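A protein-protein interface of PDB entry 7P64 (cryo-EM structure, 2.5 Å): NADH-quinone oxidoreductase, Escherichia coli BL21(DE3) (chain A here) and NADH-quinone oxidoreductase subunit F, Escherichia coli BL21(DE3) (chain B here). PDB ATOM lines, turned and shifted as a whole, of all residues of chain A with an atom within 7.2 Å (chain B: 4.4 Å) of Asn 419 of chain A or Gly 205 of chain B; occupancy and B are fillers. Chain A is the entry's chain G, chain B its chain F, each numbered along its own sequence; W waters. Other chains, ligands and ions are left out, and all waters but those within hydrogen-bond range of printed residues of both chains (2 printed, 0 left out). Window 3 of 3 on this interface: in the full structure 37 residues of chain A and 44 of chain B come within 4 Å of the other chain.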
ATOM      1  N   ALA A 400      -3.299 -21.841  24.491  1.00  0.00           N
ATOM      2  CA  ALA A 400      -1.861 -21.617  24.564  1.00  0.00           C
ATOM      3  C   ALA A 400      -1.308 -22.048  25.909  1.00  0.00           C
ATOM      4  O   ALA A 400      -0.179 -22.553  25.979  1.00  0.00           O
ATOM      5  CB  ALA A 400      -1.534 -20.149  24.311  1.00  0.00           C
ATOM      6  N   GLN A 413       5.518 -18.683  33.620  1.00  0.00           N
ATOM      7  CA  GLN A 413       6.432 -18.244  32.565  1.00  0.00           C
ATOM      8  C   GLN A 413       5.617 -17.767  31.362  1.00  0.00           C
ATOM      9  O   GLN A 413       5.544 -18.415  30.318  1.00  0.00           O
ATOM     10  CB  GLN A 413       7.379 -19.373  32.181  1.00  0.00           C
ATOM     11  CG  GLN A 413       8.830 -19.141  32.559  1.00  0.00           C
ATOM     12  CD  GLN A 413       9.649 -18.576  31.415  1.00  0.00           C
ATOM     13  OE1 GLN A 413       9.253 -17.605  30.772  1.00  0.00           O
ATOM     14  NE2 GLN A 413      10.797 -19.188  31.152  1.00  0.00           N
ATOM     15  N   ILE A 414       5.009 -16.588  31.528  1.00  0.00           N
ATOM     16  CA  ILE A 414       3.965 -16.140  30.609  1.00  0.00           C
ATOM     17  C   ILE A 414       4.524 -15.804  29.226  1.00  0.00           C
ATOM     18  O   ILE A 414       3.849 -16.026  28.213  1.00  0.00           O
ATOM     19  CB  ILE A 414       3.184 -14.963  31.235  1.00  0.00           C
ATOM     20  CG1 ILE A 414       1.982 -14.579  30.369  1.00  0.00           C
ATOM     21  CG2 ILE A 414       4.083 -13.764  31.511  1.00  0.00           C
ATOM     22  CD1 ILE A 414       1.031 -15.724  30.101  1.00  0.00           C
ATOM     23  N   ALA A 415       5.756 -15.289  29.148  1.00  0.00           N
ATOM     24  CA  ALA A 415       6.344 -14.971  27.849  1.00  0.00           C
ATOM     25  C   ALA A 415       6.575 -16.228  27.021  1.00  0.00           C
ATOM     26  O   ALA A 415       6.300 -16.243  25.816  1.00  0.00           O
ATOM     27  CB  ALA A 415       7.652 -14.204  28.033  1.00  0.00           C
ATOM     28  N   ALA A 416       7.055 -17.298  27.657  1.00  0.00           N
ATOM     29  CA  ALA A 416       7.246 -18.565  26.959  1.00  0.00           C
ATOM     30  C   ALA A 416       5.915 -19.167  26.528  1.00  0.00           C
ATOM     31  O   ALA A 416       5.817 -19.760  25.446  1.00  0.00           O
ATOM     32  CB  ALA A 416       8.011 -19.539  27.848  1.00  0.00           C
ATOM     33  N   ILE A 417       4.884 -19.027  27.367  1.00  0.00           N
ATOM     34  CA  ILE A 417       3.555 -19.532  27.033  1.00  0.00           C
ATOM     35  C   ILE A 417       3.004 -18.808  25.812  1.00  0.00           C
ATOM     36  O   ILE A 417       2.479 -19.431  24.882  1.00  0.00           O
ATOM     37  CB  ILE A 417       2.612 -19.392  28.243  1.00  0.00           C
ATOM     38  CG1 ILE A 417       3.082 -20.287  29.390  1.00  0.00           C
ATOM     39  CG2 ILE A 417       1.181 -19.717  27.859  1.00  0.00           C
ATOM     40  CD1 ILE A 417       2.318 -20.093  30.669  1.00  0.00           C
ATOM     41  N   LEU A 418       3.135 -17.479  25.787  1.00  0.00           N
ATOM     42  CA  LEU A 418       2.655 -16.707  24.648  1.00  0.00           C
ATOM     43  C   LEU A 418       3.491 -16.957  23.400  1.00  0.00           C
ATOM     44  O   LEU A 418       2.975 -16.856  22.283  1.00  0.00           O
ATOM     45  CB  LEU A 418       2.642 -15.217  24.988  1.00  0.00           C
ATOM     46  CG  LEU A 418       1.677 -14.780  26.091  1.00  0.00           C
ATOM     47  CD1 LEU A 418       1.626 -13.264  26.196  1.00  0.00           C
ATOM     48  CD2 LEU A 418       0.291 -15.359  25.866  1.00  0.00           C
ATOM     49  N   ASN A 419       4.776 -17.275  23.567  1.00  0.00           N
ATOM     50  CA  ASN A 419       5.607 -17.598  22.413  1.00  0.00           C
ATOM     51  C   ASN A 419       5.238 -18.951  21.818  1.00  0.00           C
ATOM     52  O   ASN A 419       5.255 -19.117  20.594  1.00  0.00           O
ATOM     53  CB  ASN A 419       7.083 -17.574  22.799  1.00  0.00           C
ATOM     54  CG  ASN A 419       7.987 -17.940  21.645  1.00  0.00           C
ATOM     55  OD1 ASN A 419       7.987 -17.279  20.610  1.00  0.00           O
ATOM     56  ND2 ASN A 419       8.753 -19.010  21.810  1.00  0.00           N
ATOM     57  N   ILE A 420       4.914 -19.932  22.663  1.00  0.00           N
ATOM     58  CA  ILE A 420       4.564 -21.260  22.163  1.00  0.00           C
ATOM     59  C   ILE A 420       3.210 -21.223  21.462  1.00  0.00           C
ATOM     60  O   ILE A 420       3.088 -21.593  20.289  1.00  0.00           O
ATOM     61  CB  ILE A 420       4.577 -22.290  23.306  1.00  0.00           C
ATOM     62  CG1 ILE A 420       6.012 -22.589  23.735  1.00  0.00           C
ATOM     63  CG2 ILE A 420       3.884 -23.576  22.885  1.00  0.00           C
ATOM     64  CD1 ILE A 420       6.111 -23.299  25.060  1.00  0.00           C
ATOM     65  N   GLY A 421       2.179 -20.775  22.168  1.00  0.00           N
ATOM     66  CA  GLY A 421       0.866 -20.607  21.583  1.00  0.00           C
ATOM     67  C   GLY A 421       0.724 -19.268  20.896  1.00  0.00           C
ATOM     68  O   GLY A 421       0.139 -18.341  21.465  1.00  0.00           O
ATOM     69  N   GLN A 422       1.275 -19.153  19.686  1.00  0.00           N
ATOM     70  CA  GLN A 422       1.398 -17.883  18.980  1.00  0.00           C
ATOM     71  C   GLN A 422       0.055 -17.221  18.704  1.00  0.00           C
ATOM     72  O   GLN A 422      -0.262 -16.179  19.286  1.00  0.00           O
ATOM     73  CB  GLN A 422       2.135 -18.098  17.659  1.00  0.00           C
ATOM     74  CG  GLN A 422       3.618 -18.310  17.810  1.00  0.00           C
ATOM     75  CD  GLN A 422       4.372 -17.008  17.918  1.00  0.00           C
ATOM     76  OE1 GLN A 422       4.153 -16.088  17.133  1.00  0.00           O
ATOM     77  NE2 GLN A 422       5.264 -16.919  18.893  1.00  0.00           N
ATOM     78  N   ARG A 423      -0.748 -17.827  17.838  1.00  0.00           N
ATOM     79  CA  ARG A 423      -2.078 -17.324  17.548  1.00  0.00           C
ATOM     80  C   ARG A 423      -3.147 -18.384  17.739  1.00  0.00           C
ATOM     81  O   ARG A 423      -4.326 -18.103  17.503  1.00  0.00           O
ATOM     82  CB  ARG A 423      -2.147 -16.766  16.118  1.00  0.00           C
ATOM     83  CG  ARG A 423      -1.975 -15.259  16.041  1.00  0.00           C
ATOM     84  CD  ARG A 423      -1.639 -14.793  14.632  1.00  0.00           C
ATOM     85  NE  ARG A 423      -0.802 -15.747  13.916  1.00  0.00           N
ATOM     86  CZ  ARG A 423      -0.800 -15.900  12.598  1.00  0.00           C
ATOM     87  NH1 ARG A 423      -1.582 -15.175  11.817  1.00  0.00           N
ATOM     88  NH2 ARG A 423       0.007 -16.805  12.051  1.00  0.00           N
ATOM     89  N   ILE B 184      15.254 -13.160  17.316  1.00  0.00           N
ATOM     90  CA  ILE B 184      14.006 -13.850  17.013  1.00  0.00           C
ATOM     91  C   ILE B 184      12.821 -12.905  17.176  1.00  0.00           C
ATOM     92  O   ILE B 184      11.899 -12.896  16.350  1.00  0.00           O
ATOM     93  CB  ILE B 184      13.880 -15.100  17.900  1.00  0.00           C
ATOM     94  CG1 ILE B 184      14.849 -16.180  17.428  1.00  0.00           C
ATOM     95  CG2 ILE B 184      12.475 -15.637  17.893  1.00  0.00           C
ATOM     96  CD1 ILE B 184      15.129 -17.223  18.468  1.00  0.00           C
ATOM     97  N   GLU B 188      10.247 -11.556  14.114  1.00  0.00           N
ATOM     98  CA  GLU B 188       8.798 -11.652  14.201  1.00  0.00           C
ATOM     99  C   GLU B 188       8.104 -10.304  14.088  1.00  0.00           C
ATOM    100  O   GLU B 188       6.884 -10.241  14.261  1.00  0.00           O
ATOM    101  CB  GLU B 188       8.393 -12.324  15.514  1.00  0.00           C
ATOM    102  CG  GLU B 188       8.780 -13.783  15.619  1.00  0.00           C
ATOM    103  CD  GLU B 188       8.423 -14.375  16.965  1.00  0.00           C
ATOM    104  OE1 GLU B 188       7.823 -13.656  17.787  1.00  0.00           O
ATOM    105  OE2 GLU B 188       8.744 -15.555  17.205  1.00  0.00           O
ATOM    106  N   ARG B 195      14.661 -12.733  25.340  1.00  0.00           N
ATOM    107  CA  ARG B 195      13.785 -13.650  26.047  1.00  0.00           C
ATOM    108  C   ARG B 195      14.569 -14.400  27.113  1.00  0.00           C
ATOM    109  O   ARG B 195      15.789 -14.554  27.026  1.00  0.00           O
ATOM    110  CB  ARG B 195      13.133 -14.653  25.090  1.00  0.00           C
ATOM    111  CG  ARG B 195      12.447 -14.024  23.899  1.00  0.00           C
ATOM    112  CD  ARG B 195      12.001 -15.084  22.918  1.00  0.00           C
ATOM    113  NE  ARG B 195      11.161 -14.535  21.862  1.00  0.00           N
ATOM    114  CZ  ARG B 195      10.638 -15.251  20.877  1.00  0.00           C
ATOM    115  NH1 ARG B 195      10.854 -16.551  20.778  1.00  0.00           N
ATOM    116  NH2 ARG B 195       9.883 -14.646  19.966  1.00  0.00           N
ATOM    117  N   PRO B 201      15.905 -21.371  22.253  1.00  0.00           N
ATOM    118  CA  PRO B 201      15.321 -21.329  20.901  1.00  0.00           C
ATOM    119  C   PRO B 201      15.308 -22.660  20.171  1.00  0.00           C
ATOM    120  O   PRO B 201      14.513 -22.818  19.237  1.00  0.00           O
ATOM    121  CB  PRO B 201      16.205 -20.310  20.174  1.00  0.00           C
ATOM    122  CG  PRO B 201      16.662 -19.408  21.242  1.00  0.00           C
ATOM    123  CD  PRO B 201      16.877 -20.277  22.446  1.00  0.00           C
ATOM    124  N   THR B 203      14.196 -25.396  21.360  1.00  0.00           N
ATOM    125  CA  THR B 203      12.918 -26.001  21.708  1.00  0.00           C
ATOM    126  C   THR B 203      11.747 -25.186  21.162  1.00  0.00           C
ATOM    127  O   THR B 203      10.862 -25.735  20.499  1.00  0.00           O
ATOM    128  CB  THR B 203      12.822 -26.158  23.232  1.00  0.00           C
ATOM    129  OG1 THR B 203      13.522 -27.342  23.629  1.00  0.00           O
ATOM    130  CG2 THR B 203      11.373 -26.275  23.691  1.00  0.00           C
ATOM    131  N   SER B 204      11.736 -23.875  21.413  1.00  0.00           N
ATOM    132  CA  SER B 204      10.676 -23.005  20.906  1.00  0.00           C
ATOM    133  C   SER B 204      11.306 -21.650  20.598  1.00  0.00           C
ATOM    134  O   SER B 204      11.470 -20.821  21.496  1.00  0.00           O
ATOM    135  CB  SER B 204       9.535 -22.880  21.907  1.00  0.00           C
ATOM    136  OG  SER B 204       9.943 -22.173  23.063  1.00  0.00           O
ATOM    137  N   GLY B 205      11.652 -21.436  19.333  1.00  0.00           N
ATOM    138  CA  GLY B 205      12.297 -20.206  18.928  1.00  0.00           C
ATOM    139  C   GLY B 205      11.408 -19.292  18.115  1.00  0.00           C
ATOM    140  O   GLY B 205      10.502 -18.657  18.659  1.00  0.00           O
ATOM    141  N   ALA B 206      11.654 -19.221  16.810  1.00  0.00           N
ATOM    142  CA  ALA B 206      10.918 -18.308  15.945  1.00  0.00           C
ATOM    143  C   ALA B 206       9.502 -18.820  15.730  1.00  0.00           C
ATOM    144  O   ALA B 206       9.309 -19.938  15.242  1.00  0.00           O
ATOM    145  CB  ALA B 206      11.641 -18.143  14.613  1.00  0.00           C
ATOM    146  N   TRP B 207       8.521 -17.994  16.107  1.00  0.00           N
ATOM    147  CA  TRP B 207       7.092 -18.303  16.011  1.00  0.00           C
ATOM    148  C   TRP B 207       6.733 -19.580  16.763  1.00  0.00           C
ATOM    149  O   TRP B 207       5.842 -20.326  16.352  1.00  0.00           O
ATOM    150  CB  TRP B 207       6.633 -18.386  14.552  1.00  0.00           C
ATOM    151  CG  TRP B 207       6.837 -17.116  13.793  1.00  0.00           C
ATOM    152  CD1 TRP B 207       6.089 -15.981  13.881  1.00  0.00           C
ATOM    153  CD2 TRP B 207       7.857 -16.848  12.826  1.00  0.00           C
ATOM    154  NE1 TRP B 207       6.579 -15.023  13.031  1.00  0.00           N
ATOM    155  CE2 TRP B 207       7.665 -15.531  12.370  1.00  0.00           C
ATOM    156  CE3 TRP B 207       8.914 -17.595  12.301  1.00  0.00           C
ATOM    157  CZ2 TRP B 207       8.490 -14.946  11.417  1.00  0.00           C
ATOM    158  CZ3 TRP B 207       9.731 -17.012  11.355  1.00  0.00           C
ATOM    159  CH2 TRP B 207       9.515 -15.701  10.922  1.00  0.00           C
ATOM    160  N   GLY B 208       7.430 -19.845  17.867  1.00  0.00           N
ATOM    161  CA  GLY B 208       7.201 -21.023  18.669  1.00  0.00           C
ATOM    162  C   GLY B 208       7.778 -22.303  18.111  1.00  0.00           C
ATOM    163  O   GLY B 208       7.717 -23.335  18.790  1.00  0.00           O
ATOM    164  N   LYS B 209       8.335 -22.276  16.912  1.00  0.00           N
ATOM    165  CA  LYS B 209       8.890 -23.440  16.249  1.00  0.00           C
ATOM    166  C   LYS B 209      10.334 -23.653  16.669  1.00  0.00           C
ATOM    167  O   LYS B 209      10.981 -22.737  17.182  1.00  0.00           O
ATOM    168  CB  LYS B 209       8.806 -23.270  14.736  1.00  0.00           C
ATOM    169  CG  LYS B 209       7.458 -22.795  14.247  1.00  0.00           C
ATOM    170  CD  LYS B 209       6.376 -23.813  14.537  1.00  0.00           C
ATOM    171  CE  LYS B 209       5.061 -23.396  13.910  1.00  0.00           C
ATOM    172  NZ  LYS B 209       4.552 -22.126  14.495  1.00  0.00           N
ATOM    173  N   THR B 211      14.082 -23.526  16.318  1.00  0.00           N
ATOM    174  CA  THR B 211      14.867 -22.526  15.612  1.00  0.00           C
ATOM    175  C   THR B 211      16.314 -22.631  16.062  1.00  0.00           C
ATOM    176  O   THR B 211      16.590 -22.797  17.252  1.00  0.00           O
ATOM    177  CB  THR B 211      14.333 -21.114  15.892  1.00  0.00           C
ATOM    178  OG1 THR B 211      12.922 -21.079  15.651  1.00  0.00           O
ATOM    179  CG2 THR B 211      15.004 -20.097  15.006  1.00  0.00           C
HETATM  180  O   HOH W   1       4.916 -13.416  16.654  1.00  0.00           O
HETATM  181  O   HOH W   2       6.460 -14.475  20.557  1.00  0.00           O
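O of Ser 204 of chain B sits at hydrogen-bond distance from ND2 of Asn 419 of chain A (3.3 Å). The backbone carbonyl oxygen (O) of Gly 205 of chain B lies close to the side-chain amide oxygen (OD1) of Asn 419 of chain A, 3.5 Å away. The side-chain amide oxygen of Asn 419 of chain A is in hydrogen-bond range of the guanidinium group of Arg 195 of chain B, 3.0 Å away.
O of Trp 207 of chain B is in hydrogen-bond range of NZ of Lys 209 of chain B (2.9 Å). The side-chain carboxylate of Glu 188 of chain B lies within hydrogen-bond range of the backbone NH of Trp 207 of chain B, 2.7 Å away. The side-chain carboxylate (OE2) of Glu 188 of chain B is in salt-bridge range of the guanidinium group (NH2) of Arg 195 of chain B (3.1 Å). The side-chain amide nitrogen of Gln 422 of chain A sits at hydrogen-bond distance from the backbone carbonyl oxygen of Asn 419 of chain A (2.8 Å). The guanidinium group (NH1) of Arg 195 of chain B lies within hydrogen-bond range of the backbone carbonyl oxygen (O) of Gly 205 of chain B, at 3.0 Å.
Among the printed residues, pairs that only touch across the chains: Asn 419 of chain A with Gly 208 of chain B (3.3 Å), Gln 422 of chain A with Trp 207 of chain B (3.3 Å), Gln 422 of chain A with Gly 208 of chain B (3.8 Å), Asn 419 of chain A with Glu 188 of chain B (3.9 Å) and Ile 420 of chain A with Ser 204 of chain B (3.98 Å).
Asn 419 of chain A touches just these residues of chain B: Glu 188, Arg 195, Ser 204, Gly 205 and Gly 208. Printed residues of chain B within 4 Å of Gln 422 of chain A: Trp 207 and Gly 208. Ile 184 of chain B touches none of the printed residues of chain A. Printed residues of chain A within 4 Å of Glu 188 of chain B: Asn 419 (3.9 Å). Printed residues of chain A within 4 Å of Arg 195 of chain B: Asn 419. Pro 201 of chain B touches none of the printed residues of chain A. Printed residues of chain A within 4 Å of Ser 204 of chain B: Asn 419 and Ile 420. Of the printed residues of chain A, Gly 208 of chain B touches Asn 419 (3.3 Å) and Gln 422 (3.8 Å). The nearest residue of chain A that does not touch Gly 205 of chain B is Gln 422 of chain A (5.5 Å). The nearest printed residue of chain A that does not touch Glu 188 of chain B is Gln 422 of chain A (4.1 Å).
Of the 12 printed residues of chain A, 3 touch a printed residue of chain B. Printed residues of chain A that touch a printed residue of chain B: Asn 419, Ile 420 and Gln 422. Printed residues of chain B that touch a printed residue of chain A: Glu 188, Arg 195, Ser 204, Gly 205, Trp 207 and Gly 208. Hydrophobic or aromatic side chains of chain B within 4 Å of the printed part of chain A: Trp 207. Among the printed residues, 8 pairs touch across the chains. Among the printed residues, no Asp or Glu carboxylate lies within 4 Å of a Lys or Arg side-chain nitrogen of the other chain.
Water W1 lies within hydrogen-bond range of OE1 of Gln 422 of chain A (2.8 Å) and OE1 of Glu 188 of chain B (3.1 Å). Water W2 lies within hydrogen-bond range of NE2 of Gln 422 of chain A, OD1 of Asn 419 of chain A, OE1 of Glu 188 of chain B and NH2 of Arg 195 of chain B.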
